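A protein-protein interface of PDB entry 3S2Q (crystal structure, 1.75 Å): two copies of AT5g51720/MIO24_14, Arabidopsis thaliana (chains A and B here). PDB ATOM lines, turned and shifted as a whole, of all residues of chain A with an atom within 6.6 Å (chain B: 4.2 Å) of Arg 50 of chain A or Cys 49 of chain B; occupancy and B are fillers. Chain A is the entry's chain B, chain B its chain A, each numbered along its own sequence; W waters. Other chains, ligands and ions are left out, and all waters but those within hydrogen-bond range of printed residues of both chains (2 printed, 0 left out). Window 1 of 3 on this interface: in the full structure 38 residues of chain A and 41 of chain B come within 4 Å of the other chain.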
ATOM      1  N   ILE A  21       0.171  -7.877 -23.716  1.00  0.00           N
ATOM      2  CA  ILE A  21      -0.861  -8.802 -23.216  1.00  0.00           C
ATOM      3  C   ILE A  21      -2.125  -8.067 -22.755  1.00  0.00           C
ATOM      4  O   ILE A  21      -3.180  -8.680 -22.526  1.00  0.00           O
ATOM      5  CB  ILE A  21      -0.317  -9.730 -22.109  1.00  0.00           C
ATOM      6  CG1 ILE A  21      -0.206  -8.998 -20.783  1.00  0.00           C
ATOM      7  CG2 ILE A  21       1.055 -10.348 -22.504  1.00  0.00           C
ATOM      8  CD1 ILE A  21       0.353  -9.846 -19.653  1.00  0.00           C
ATOM      9  N   TYR A  48      -8.611 -12.744  -8.361  1.00  0.00           N
ATOM     10  CA  TYR A  48      -7.981 -11.594  -9.006  1.00  0.00           C
ATOM     11  C   TYR A  48      -7.566 -11.951 -10.412  1.00  0.00           C
ATOM     12  O   TYR A  48      -7.056 -13.056 -10.663  1.00  0.00           O
ATOM     13  CB  TYR A  48      -6.802 -11.077  -8.172  1.00  0.00           C
ATOM     14  CG  TYR A  48      -7.301 -10.175  -7.060  1.00  0.00           C
ATOM     15  CD1 TYR A  48      -7.213  -8.787  -7.181  1.00  0.00           C
ATOM     16  CD2 TYR A  48      -7.914 -10.716  -5.890  1.00  0.00           C
ATOM     17  CE1 TYR A  48      -7.713  -7.938  -6.181  1.00  0.00           C
ATOM     18  CE2 TYR A  48      -8.429  -9.865  -4.880  1.00  0.00           C
ATOM     19  CZ  TYR A  48      -8.326  -8.484  -5.041  1.00  0.00           C
ATOM     20  OH  TYR A  48      -8.789  -7.609  -4.075  1.00  0.00           O
ATOM     21  N   CYS A  49      -7.796 -11.015 -11.331  1.00  0.00           N
ATOM     22  CA  CYS A  49      -7.591 -11.244 -12.761  1.00  0.00           C
ATOM     23  C   CYS A  49      -6.116 -11.251 -13.182  1.00  0.00           C
ATOM     24  O   CYS A  49      -5.356 -10.381 -12.776  1.00  0.00           O
ATOM     25  CB  CYS A  49      -8.271 -10.133 -13.530  1.00  0.00           C
ATOM     26  SG  CYS A  49      -8.149 -10.295 -15.324  1.00  0.00           S
ATOM     27  N   ARG A  50      -5.726 -12.254 -13.973  1.00  0.00           N
ATOM     28  CA  ARG A  50      -4.350 -12.340 -14.527  1.00  0.00           C
ATOM     29  C   ARG A  50      -4.388 -12.368 -16.064  1.00  0.00           C
ATOM     30  O   ARG A  50      -3.359 -12.626 -16.724  1.00  0.00           O
ATOM     31  CB  ARG A  50      -3.585 -13.547 -13.978  1.00  0.00           C
ATOM     32  CG  ARG A  50      -3.374 -13.456 -12.439  1.00  0.00           C
ATOM     33  CD  ARG A  50      -2.455 -14.542 -11.920  1.00  0.00           C
ATOM     34  NE  ARG A  50      -2.931 -15.904 -12.210  1.00  0.00           N
ATOM     35  CZ  ARG A  50      -2.374 -17.017 -11.711  1.00  0.00           C
ATOM     36  NH1 ARG A  50      -1.336 -16.953 -10.877  1.00  0.00           N
ATOM     37  NH2 ARG A  50      -2.855 -18.204 -12.039  1.00  0.00           N
ATOM     38  N   CYS A  51      -5.577 -12.111 -16.616  1.00  0.00           N
ATOM     39  CA  CYS A  51      -5.789 -12.159 -18.089  1.00  0.00           C
ATOM     40  C   CYS A  51      -5.977 -10.797 -18.729  1.00  0.00           C
ATOM     41  O   CYS A  51      -5.982 -10.684 -19.957  1.00  0.00           O
ATOM     42  CB  CYS A  51      -6.975 -13.066 -18.449  1.00  0.00           C
ATOM     43  SG  CYS A  51      -8.637 -12.352 -18.281  1.00  0.00           S
ATOM     44  N   TRP A  52      -6.169  -9.762 -17.909  1.00  0.00           N
ATOM     45  CA  TRP A  52      -6.303  -8.381 -18.437  1.00  0.00           C
ATOM     46  C   TRP A  52      -7.554  -8.196 -19.311  1.00  0.00           C
ATOM     47  O   TRP A  52      -7.605  -7.281 -20.112  1.00  0.00           O
ATOM     48  CB  TRP A  52      -5.009  -7.924 -19.177  1.00  0.00           C
ATOM     49  CG  TRP A  52      -3.851  -7.965 -18.248  1.00  0.00           C
ATOM     50  CD1 TRP A  52      -3.039  -9.049 -17.980  1.00  0.00           C
ATOM     51  CD2 TRP A  52      -3.418  -6.909 -17.376  1.00  0.00           C
ATOM     52  NE1 TRP A  52      -2.131  -8.719 -17.001  1.00  0.00           N
ATOM     53  CE2 TRP A  52      -2.326  -7.416 -16.619  1.00  0.00           C
ATOM     54  CE3 TRP A  52      -3.810  -5.572 -17.193  1.00  0.00           C
ATOM     55  CZ2 TRP A  52      -1.628  -6.632 -15.675  1.00  0.00           C
ATOM     56  CZ3 TRP A  52      -3.117  -4.789 -16.235  1.00  0.00           C
ATOM     57  CH2 TRP A  52      -2.039  -5.332 -15.492  1.00  0.00           C
ATOM     58  N   ARG A  53      -8.571  -9.055 -19.141  1.00  0.00           N
ATOM     59  CA  ARG A  53      -9.836  -8.931 -19.895  1.00  0.00           C
ATOM     60  C   ARG A  53     -11.029  -8.633 -18.979  1.00  0.00           C
ATOM     61  O   ARG A  53     -12.123  -8.314 -19.478  1.00  0.00           O
ATOM     62  CB  ARG A  53     -10.170 -10.222 -20.687  1.00  0.00           C
ATOM     63  CG  ARG A  53      -9.091 -10.811 -21.636  1.00  0.00           C
ATOM     64  CD  ARG A  53      -8.521  -9.744 -22.462  1.00  0.00           C
ATOM     65  NE  ARG A  53      -7.739 -10.129 -23.655  1.00  0.00           N
ATOM     66  CZ  ARG A  53      -6.413 -10.152 -23.721  1.00  0.00           C
ATOM     67  NH1 ARG A  53      -5.682  -9.932 -22.636  1.00  0.00           N
ATOM     68  NH2 ARG A  53      -5.811 -10.396 -24.890  1.00  0.00           N
ATOM     69  N   PHE A  57     -11.612  -5.581 -13.470  1.00  0.00           N
ATOM     70  CA  PHE A  57     -10.188  -5.602 -13.170  1.00  0.00           C
ATOM     71  C   PHE A  57      -9.892  -4.570 -12.067  1.00  0.00           C
ATOM     72  O   PHE A  57     -10.329  -3.442 -12.181  1.00  0.00           O
ATOM     73  CB  PHE A  57      -9.384  -5.208 -14.424  1.00  0.00           C
ATOM     74  CG  PHE A  57      -7.898  -5.502 -14.295  1.00  0.00           C
ATOM     75  CD1 PHE A  57      -7.018  -4.568 -13.749  1.00  0.00           C
ATOM     76  CD2 PHE A  57      -7.405  -6.741 -14.681  1.00  0.00           C
ATOM     77  CE1 PHE A  57      -5.653  -4.876 -13.605  1.00  0.00           C
ATOM     78  CE2 PHE A  57      -6.058  -7.051 -14.563  1.00  0.00           C
ATOM     79  CZ  PHE A  57      -5.178  -6.126 -14.003  1.00  0.00           C
ATOM     80  N   PRO A  58      -9.073  -4.916 -11.055  1.00  0.00           N
ATOM     81  CA  PRO A  58      -8.197  -6.101 -10.915  1.00  0.00           C
ATOM     82  C   PRO A  58      -8.890  -7.392 -10.467  1.00  0.00           C
ATOM     83  O   PRO A  58      -8.235  -8.436 -10.400  1.00  0.00           O
ATOM     84  CB  PRO A  58      -7.180  -5.650  -9.858  1.00  0.00           C
ATOM     85  CG  PRO A  58      -7.989  -4.651  -9.001  1.00  0.00           C
ATOM     86  CD  PRO A  58      -8.794  -3.895 -10.030  1.00  0.00           C
ATOM     87  N   CYS A  60     -11.241 -10.720 -10.895  1.00  0.00           N
ATOM     88  CA  CYS A  60     -11.625 -11.659 -11.945  1.00  0.00           C
ATOM     89  C   CYS A  60     -13.139 -11.772 -12.046  1.00  0.00           C
ATOM     90  O   CYS A  60     -13.795 -12.052 -11.047  1.00  0.00           O
ATOM     91  CB  CYS A  60     -11.030 -13.035 -11.621  1.00  0.00           C
ATOM     92  SG  CYS A  60     -11.669 -14.393 -12.642  1.00  0.00           S
ATOM     93  N   VAL A  75      -4.954 -19.335 -19.293  1.00  0.00           N
ATOM     94  CA  VAL A  75      -4.716 -18.436 -18.154  1.00  0.00           C
ATOM     95  C   VAL A  75      -5.931 -18.437 -17.217  1.00  0.00           C
ATOM     96  O   VAL A  75      -7.055 -18.686 -17.650  1.00  0.00           O
ATOM     97  CB  VAL A  75      -4.341 -16.983 -18.588  1.00  0.00           C
ATOM     98  CG1 VAL A  75      -2.972 -16.962 -19.261  1.00  0.00           C
ATOM     99  CG2 VAL A  75      -5.412 -16.328 -19.489  1.00  0.00           C
ATOM    100  N   GLY A  76      -5.670 -18.209 -15.928  1.00  0.00           N
ATOM    101  CA  GLY A  76      -6.734 -18.151 -14.945  1.00  0.00           C
ATOM    102  C   GLY A  76      -6.342 -17.251 -13.779  1.00  0.00           C
ATOM    103  O   GLY A  76      -5.219 -16.739 -13.706  1.00  0.00           O
ATOM    104  N   PRO A  77      -7.292 -17.022 -12.878  1.00  0.00           N
ATOM    105  CA  PRO A  77      -7.138 -16.078 -11.784  1.00  0.00           C
ATOM    106  C   PRO A  77      -6.185 -16.523 -10.649  1.00  0.00           C
ATOM    107  O   PRO A  77      -5.812 -17.704 -10.560  1.00  0.00           O
ATOM    108  CB  PRO A  77      -8.596 -15.926 -11.274  1.00  0.00           C
ATOM    109  CG  PRO A  77      -9.226 -17.210 -11.557  1.00  0.00           C
ATOM    110  CD  PRO A  77      -8.622 -17.662 -12.882  1.00  0.00           C
ATOM    111  N   LEU A  78      -5.794 -15.555  -9.817  1.00  0.00           N
ATOM    112  CA  LEU A  78      -5.124 -15.801  -8.550  1.00  0.00           C
ATOM    113  C   LEU A  78      -6.177 -15.746  -7.441  1.00  0.00           C
ATOM    114  O   LEU A  78      -6.919 -14.759  -7.333  1.00  0.00           O
ATOM    115  CB  LEU A  78      -4.074 -14.732  -8.311  1.00  0.00           C
ATOM    116  CG  LEU A  78      -3.216 -14.918  -7.048  1.00  0.00           C
ATOM    117  CD1 LEU A  78      -2.307 -16.154  -7.146  1.00  0.00           C
ATOM    118  CD2 LEU A  78      -2.379 -13.667  -6.785  1.00  0.00           C
ATOM    119  N   LEU A  79      -6.247 -16.806  -6.638  1.00  0.00           N
ATOM    120  CA  LEU A  79      -7.292 -16.901  -5.612  1.00  0.00           C
ATOM    121  C   LEU A  79      -6.735 -16.502  -4.236  1.00  0.00           C
ATOM    122  O   LEU A  79      -5.874 -17.189  -3.695  1.00  0.00           O
ATOM    123  CB  LEU A  79      -7.839 -18.324  -5.548  1.00  0.00           C
ATOM    124  CG  LEU A  79      -8.402 -18.950  -6.840  1.00  0.00           C
ATOM    125  CD1 LEU A  79      -9.131 -20.274  -6.527  1.00  0.00           C
ATOM    126  CD2 LEU A  79      -9.344 -18.020  -7.605  1.00  0.00           C
ATOM    127  N   ILE B  21      -1.706 -15.090 -24.197  1.00  0.00           N
ATOM    128  CA  ILE B  21      -0.846 -14.224 -23.399  1.00  0.00           C
ATOM    129  C   ILE B  21       0.173 -15.010 -22.583  1.00  0.00           C
ATOM    130  O   ILE B  21       1.093 -14.416 -22.036  1.00  0.00           O
ATOM    131  CB  ILE B  21      -1.656 -13.274 -22.472  1.00  0.00           C
ATOM    132  CG1 ILE B  21      -2.375 -14.063 -21.359  1.00  0.00           C
ATOM    133  CG2 ILE B  21      -2.613 -12.423 -23.300  1.00  0.00           C
ATOM    134  CD1 ILE B  21      -2.949 -13.155 -20.240  1.00  0.00           C
ATOM    135  N   VAL B  32      -4.580 -22.368 -15.778  1.00  0.00           N
ATOM    136  CA  VAL B  32      -3.613 -22.164 -14.692  1.00  0.00           C
ATOM    137  C   VAL B  32      -4.222 -21.237 -13.622  1.00  0.00           C
ATOM    138  O   VAL B  32      -4.417 -20.052 -13.864  1.00  0.00           O
ATOM    139  CB  VAL B  32      -2.269 -21.578 -15.215  1.00  0.00           C
ATOM    140  CG1 VAL B  32      -1.326 -21.278 -14.035  1.00  0.00           C
ATOM    141  CG2 VAL B  32      -1.611 -22.530 -16.267  1.00  0.00           C
ATOM    142  N   VAL B  33      -4.494 -21.804 -12.438  1.00  0.00           N
ATOM    143  CA  VAL B  33      -5.054 -21.082 -11.301  1.00  0.00           C
ATOM    144  C   VAL B  33      -4.108 -21.306 -10.133  1.00  0.00           C
ATOM    145  O   VAL B  33      -3.523 -22.376 -10.006  1.00  0.00           O
ATOM    146  CB  VAL B  33      -6.508 -21.584 -10.985  1.00  0.00           C
ATOM    147  CG1 VAL B  33      -7.060 -20.918  -9.756  1.00  0.00           C
ATOM    148  CG2 VAL B  33      -7.445 -21.312 -12.164  1.00  0.00           C
ATOM    149  N   ASP B  34      -3.896 -20.280  -9.323  1.00  0.00           N
ATOM    150  CA  ASP B  34      -3.050 -20.402  -8.142  1.00  0.00           C
ATOM    151  C   ASP B  34      -3.782 -19.848  -6.956  1.00  0.00           C
ATOM    152  O   ASP B  34      -4.602 -18.934  -7.103  1.00  0.00           O
ATOM    153  CB  ASP B  34      -1.739 -19.630  -8.339  1.00  0.00           C
ATOM    154  CG  ASP B  34      -0.884 -20.236  -9.433  1.00  0.00           C
ATOM    155  OD1 ASP B  34      -0.283 -21.293  -9.170  1.00  0.00           O
ATOM    156  OD2 ASP B  34      -0.844 -19.664 -10.540  1.00  0.00           O
ATOM    157  N   TYR B  48       2.791 -10.590  -6.942  1.00  0.00           N
ATOM    158  CA  TYR B  48       2.341 -11.733  -7.701  1.00  0.00           C
ATOM    159  C   TYR B  48       2.265 -11.358  -9.165  1.00  0.00           C
ATOM    160  O   TYR B  48       1.840 -10.258  -9.513  1.00  0.00           O
ATOM    161  CB  TYR B  48       0.995 -12.278  -7.164  1.00  0.00           C
ATOM    162  CG  TYR B  48       1.259 -13.179  -5.979  1.00  0.00           C
ATOM    163  CD1 TYR B  48       1.245 -14.564  -6.130  1.00  0.00           C
ATOM    164  CD2 TYR B  48       1.596 -12.648  -4.726  1.00  0.00           C
ATOM    165  CE1 TYR B  48       1.542 -15.405  -5.077  1.00  0.00           C
ATOM    166  CE2 TYR B  48       1.867 -13.495  -3.636  1.00  0.00           C
ATOM    167  CZ  TYR B  48       1.837 -14.873  -3.836  1.00  0.00           C
ATOM    168  OH  TYR B  48       2.087 -15.761  -2.817  1.00  0.00           O
ATOM    169  N   CYS B  49       2.718 -12.282 -10.008  1.00  0.00           N
ATOM    170  CA  CYS B  49       2.844 -12.031 -11.442  1.00  0.00           C
ATOM    171  C   CYS B  49       1.494 -11.994 -12.186  1.00  0.00           C
ATOM    172  O   CYS B  49       0.610 -12.869 -11.978  1.00  0.00           O
ATOM    173  CB  CYS B  49       3.830 -13.061 -12.046  1.00  0.00           C
ATOM    174  SG  CYS B  49       4.019 -12.893 -13.825  1.00  0.00           S
ATOM    175  N   ARG B  50       1.334 -10.959 -13.021  1.00  0.00           N
ATOM    176  CA  ARG B  50       0.179 -10.815 -13.913  1.00  0.00           C
ATOM    177  C   ARG B  50       0.592 -10.781 -15.377  1.00  0.00           C
ATOM    178  O   ARG B  50      -0.239 -10.607 -16.277  1.00  0.00           O
ATOM    179  CB  ARG B  50      -0.664  -9.594 -13.525  1.00  0.00           C
ATOM    180  CG  ARG B  50      -1.247  -9.734 -12.098  1.00  0.00           C
ATOM    181  CD  ARG B  50      -2.312  -8.663 -11.786  1.00  0.00           C
ATOM    182  NE  ARG B  50      -1.781  -7.289 -11.820  1.00  0.00           N
ATOM    183  CZ  ARG B  50      -2.466  -6.192 -11.471  1.00  0.00           C
ATOM    184  NH1 ARG B  50      -3.702  -6.297 -11.008  1.00  0.00           N
ATOM    185  NH2 ARG B  50      -1.909  -4.976 -11.556  1.00  0.00           N
ATOM    186  N   CYS B  51       1.884 -10.975 -15.623  1.00  0.00           N
ATOM    187  CA  CYS B  51       2.372 -10.872 -17.008  1.00  0.00           C
ATOM    188  C   CYS B  51       2.723 -12.220 -17.672  1.00  0.00           C
ATOM    189  O   CYS B  51       2.963 -12.264 -18.879  1.00  0.00           O
ATOM    190  CB  CYS B  51       3.563  -9.942 -17.081  1.00  0.00           C
ATOM    191  SG  CYS B  51       5.108 -10.691 -16.500  1.00  0.00           S
ATOM    192  N   TRP B  52       2.768 -13.289 -16.881  1.00  0.00           N
ATOM    193  CA  TRP B  52       3.016 -14.673 -17.369  1.00  0.00           C
ATOM    194  C   TRP B  52       4.450 -14.841 -17.879  1.00  0.00           C
ATOM    195  O   TRP B  52       4.749 -15.755 -18.678  1.00  0.00           O
ATOM    196  CB  TRP B  52       1.944 -15.148 -18.392  1.00  0.00           C
ATOM    197  CG  TRP B  52       0.563 -15.128 -17.741  1.00  0.00           C
ATOM    198  CD1 TRP B  52      -0.281 -14.046 -17.617  1.00  0.00           C
ATOM    199  CD2 TRP B  52      -0.076 -16.220 -17.061  1.00  0.00           C
ATOM    200  NE1 TRP B  52      -1.420 -14.411 -16.899  1.00  0.00           N
ATOM    201  CE2 TRP B  52      -1.315 -15.732 -16.545  1.00  0.00           C
ATOM    202  CE3 TRP B  52       0.266 -17.570 -16.855  1.00  0.00           C
ATOM    203  CZ2 TRP B  52      -2.216 -16.550 -15.835  1.00  0.00           C
ATOM    204  CZ3 TRP B  52      -0.631 -18.395 -16.141  1.00  0.00           C
ATOM    205  CH2 TRP B  52      -1.858 -17.876 -15.642  1.00  0.00           C
ATOM    206  N   ARG B  53       5.336 -13.977 -17.402  1.00  0.00           N
ATOM    207  CA  ARG B  53       6.755 -14.051 -17.793  1.00  0.00           C
ATOM    208  C   ARG B  53       7.691 -14.331 -16.643  1.00  0.00           C
ATOM    209  O   ARG B  53       8.901 -14.457 -16.855  1.00  0.00           O
ATOM    210  CB  ARG B  53       7.211 -12.779 -18.530  1.00  0.00           C
ATOM    211  CG  ARG B  53       6.358 -12.364 -19.769  1.00  0.00           C
ATOM    212  CD  ARG B  53       6.394 -13.404 -20.837  1.00  0.00           C
ATOM    213  NE  ARG B  53       5.757 -12.998 -22.102  1.00  0.00           N
ATOM    214  CZ  ARG B  53       4.447 -13.078 -22.357  1.00  0.00           C
ATOM    215  NH1 ARG B  53       3.598 -13.546 -21.437  1.00  0.00           N
ATOM    216  NH2 ARG B  53       3.978 -12.728 -23.547  1.00  0.00           N
ATOM    217  N   SER B  54       7.166 -14.415 -15.416  1.00  0.00           N
ATOM    218  CA  SER B  54       8.055 -14.612 -14.246  1.00  0.00           C
ATOM    219  C   SER B  54       8.643 -16.012 -14.179  1.00  0.00           C
ATOM    220  O   SER B  54       7.925 -16.999 -14.351  1.00  0.00           O
ATOM    221  CB  SER B  54       7.320 -14.321 -12.935  1.00  0.00           C
ATOM    222  OG  SER B  54       8.157 -14.634 -11.802  1.00  0.00           O
ATOM    223  N   PHE B  57       6.861 -17.628 -11.229  1.00  0.00           N
ATOM    224  CA  PHE B  57       5.406 -17.669 -11.324  1.00  0.00           C
ATOM    225  C   PHE B  57       4.867 -18.747 -10.400  1.00  0.00           C
ATOM    226  O   PHE B  57       5.361 -19.879 -10.429  1.00  0.00           O
ATOM    227  CB  PHE B  57       4.974 -17.985 -12.758  1.00  0.00           C
ATOM    228  CG  PHE B  57       3.550 -17.668 -13.017  1.00  0.00           C
ATOM    229  CD1 PHE B  57       3.194 -16.397 -13.435  1.00  0.00           C
ATOM    230  CD2 PHE B  57       2.554 -18.607 -12.772  1.00  0.00           C
ATOM    231  CE1 PHE B  57       1.850 -16.059 -13.659  1.00  0.00           C
ATOM    232  CE2 PHE B  57       1.204 -18.289 -12.975  1.00  0.00           C
ATOM    233  CZ  PHE B  57       0.851 -17.019 -13.425  1.00  0.00           C
ATOM    234  N   PRO B  58       3.814 -18.434  -9.614  1.00  0.00           N
ATOM    235  CA  PRO B  58       2.970 -17.218  -9.649  1.00  0.00           C
ATOM    236  C   PRO B  58       3.553 -15.949  -9.001  1.00  0.00           C
ATOM    237  O   PRO B  58       2.940 -14.895  -9.075  1.00  0.00           O
ATOM    238  CB  PRO B  58       1.689 -17.675  -8.936  1.00  0.00           C
ATOM    239  CG  PRO B  58       2.193 -18.690  -7.933  1.00  0.00           C
ATOM    240  CD  PRO B  58       3.385 -19.374  -8.551  1.00  0.00           C
ATOM    241  N   LEU B  59       4.737 -16.029  -8.401  1.00  0.00           N
ATOM    242  CA  LEU B  59       5.346 -14.830  -7.834  1.00  0.00           C
ATOM    243  C   LEU B  59       5.900 -13.967  -8.983  1.00  0.00           C
ATOM    244  O   LEU B  59       6.211 -14.491 -10.070  1.00  0.00           O
ATOM    245  CB  LEU B  59       6.472 -15.192  -6.857  1.00  0.00           C
ATOM    246  CG  LEU B  59       6.088 -15.843  -5.513  1.00  0.00           C
ATOM    247  CD1 LEU B  59       7.346 -16.293  -4.746  1.00  0.00           C
ATOM    248  CD2 LEU B  59       5.265 -14.878  -4.670  1.00  0.00           C
ATOM    249  N   CYS B  60       5.991 -12.666  -8.741  1.00  0.00           N
ATOM    250  CA  CYS B  60       6.587 -11.711  -9.668  1.00  0.00           C
ATOM    251  C   CYS B  60       8.085 -11.672  -9.391  1.00  0.00           C
ATOM    252  O   CYS B  60       8.498 -11.623  -8.227  1.00  0.00           O
ATOM    253  CB  CYS B  60       5.974 -10.330  -9.465  1.00  0.00           C
ATOM    254  SG  CYS B  60       6.802  -8.950 -10.329  1.00  0.00           S
HETATM  255  O   HOH W   1      -5.409  -8.596 -10.649  1.00  0.00           O
HETATM  256  O   HOH W   2       0.280 -14.684 -10.017  1.00  0.00           O
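The backbone carbonyl oxygen (O) of Arg 50 of chain B is in hydrogen-bond range of the indole nitrogen (NE1) of Trp 52 of chain A (2.8 Å).
NE1 of Trp 52 of chain B lies within hydrogen-bond range of O of Arg 50 of chain A, at 2.6 Å.
The backbone carbonyl oxygen (O) of Asp 34 of chain B lies within hydrogen-bond range of the backbone NH (N) of Leu 79 of chain A (2.7 Å).
The backbone carbonyl oxygen of Pro 77 of chain A is in hydrogen-bond range of the backbone NH of Asp 34 of chain B (3.4 Å).
O of Val 32 of chain B sits at hydrogen-bond distance from NH2 of Arg 50 of chain A (3.0 Å).
The side-chain carboxylate of Asp 34 of chain B lies within salt-bridge range of the guanidinium group of Arg 50 of chain A (2.8 Å).
O of Val 32 of chain B sits at hydrogen-bond distance from N of Gly 76 of chain A (3.0 Å).
The backbone NH (N) of Cys 49 of chain B is in hydrogen-bond range of the backbone carbonyl oxygen (O) of Pro 58 of chain B.
O of Cys 51 of chain B sits at hydrogen-bond distance from NH1 of Arg 53 of chain B (2.9 Å).
The side-chain sulfur (SG) of Cys 49 of chain A lies close to the backbone NH (N) of Trp 52 of chain A (3.3 Å).
O of Gly 76 of chain A is in hydrogen-bond range of NE of Arg 50 of chain A (2.9 Å).
The guanidinium group (NH1) of Arg 53 of chain B sits at hydrogen-bond distance from the backbone carbonyl oxygen (O) of Ile 21 of chain B (2.7 Å).
O of Ile 21 of chain A lies within hydrogen-bond range of NH1 of Arg 53 of chain A.
Cys 51 of chain B touches Ile 21 of chain A.
Arg 53 of chain B touches Ile 21 of chain A.
Arg 50 of chain A touches Cys 49 of chain B (CD to O, 3.5 Å).
CB of Pro 58 of chain A touches NH1 of Arg 50 of chain B, at 3.7 Å.
Ile 21 of chain B touches Val 75 of chain A (CG1 to CG1, 3.6 Å).
CG1 of Val 75 of chain A touches CE2 of Trp 52 of chain B (3.4 Å).
O of Gly 76 of chain A touches CZ2 of Trp 52 of chain B, at 3.7 Å.
Pro 77 of chain A touches Val 33 of chain B (O to CG1, 3.5 Å).
Leu 78 of chain A touches Asp 34 of chain B (CA to O, 3.5 Å).
Leu 79 of chain A touches Val 33 of chain B (CG to CG1, 3.8 Å).
Of chain B, only Ile 21 (3.6 Å), Val 32 (3.0 Å), Val 33 (3.7 Å), Asp 34 (2.8 Å), Cys 49 (3.5 Å), Arg 50 (3.7 Å), Trp 52 (2.6 Å), Phe 57 (3.4 Å) and Pro 58 (3.7 Å) come within 4 Å of Arg 50 of chain A.
Of the printed residues of chain B, Cys 51 of chain A touches Ile 21 (3.7 Å).
Printed residues of chain A within 4 Å of Val 33 of chain B: Arg 50 (3.7 Å), Pro 77 (3.5 Å) and Leu 79 (3.8 Å).
Of the printed residues of chain A, Phe 57 of chain B touches Arg 50.
Arg 53 of chain A touches none of the printed residues of chain B.
Hydrophobic or aromatic side chains of chain A within 4 Å of the printed part of chain B: Ile 21, Trp 52, Phe 57, Pro 58, Val 75, Pro 77, Leu 78 and Leu 79.
Hydrophobic or aromatic side chains of chain B that line the printed part of chain A: Ile 21, Val 32, Val 33, Tyr 48, Trp 52, Phe 57 and Pro 58.
Along chain B the printed residues that touch a printed residue of chain A span positions 21 to 58.
Ile 21 of chain B touches its own counterpart, Ile 21 of chain A.
Ile 21 of chain A touches Cys 51 of chain B, and with the chains exchanged Cys 51 of chain A touches Ile 21 of chain B.
Arg 50 of chain A touches Trp 52 of chain B, and with the chains exchanged Trp 52 of chain A touches Arg 50 of chain B.
Arg 50 of chain A touches Pro 58 of chain B, and with the chains exchanged Pro 58 of chain A touches Arg 50 of chain B.
Positions printed for both chains: 21, 48, 49, 50, 51, 52, 53, 57, 58 and 60.
Of the 28 pairs that touch across the chains among the printed residues, 14 have their exchanged pair printed and touching as well.
Water W2 lies within hydrogen-bond range of the backbone carbonyl oxygen of Cys 49 of chain B (2.7 Å), the backbone carbonyl oxygen of Pro 58 of chain B (2.8 Å) and the guanidinium group of Arg 50 of chain A (2.9 Å).
Water W1 lies within hydrogen-bond range of O of Cys 49 of chain A (2.8 Å), O of Pro 58 of chain A (2.8 Å) and NH1 of Arg 50 of chain B (2.9 Å).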
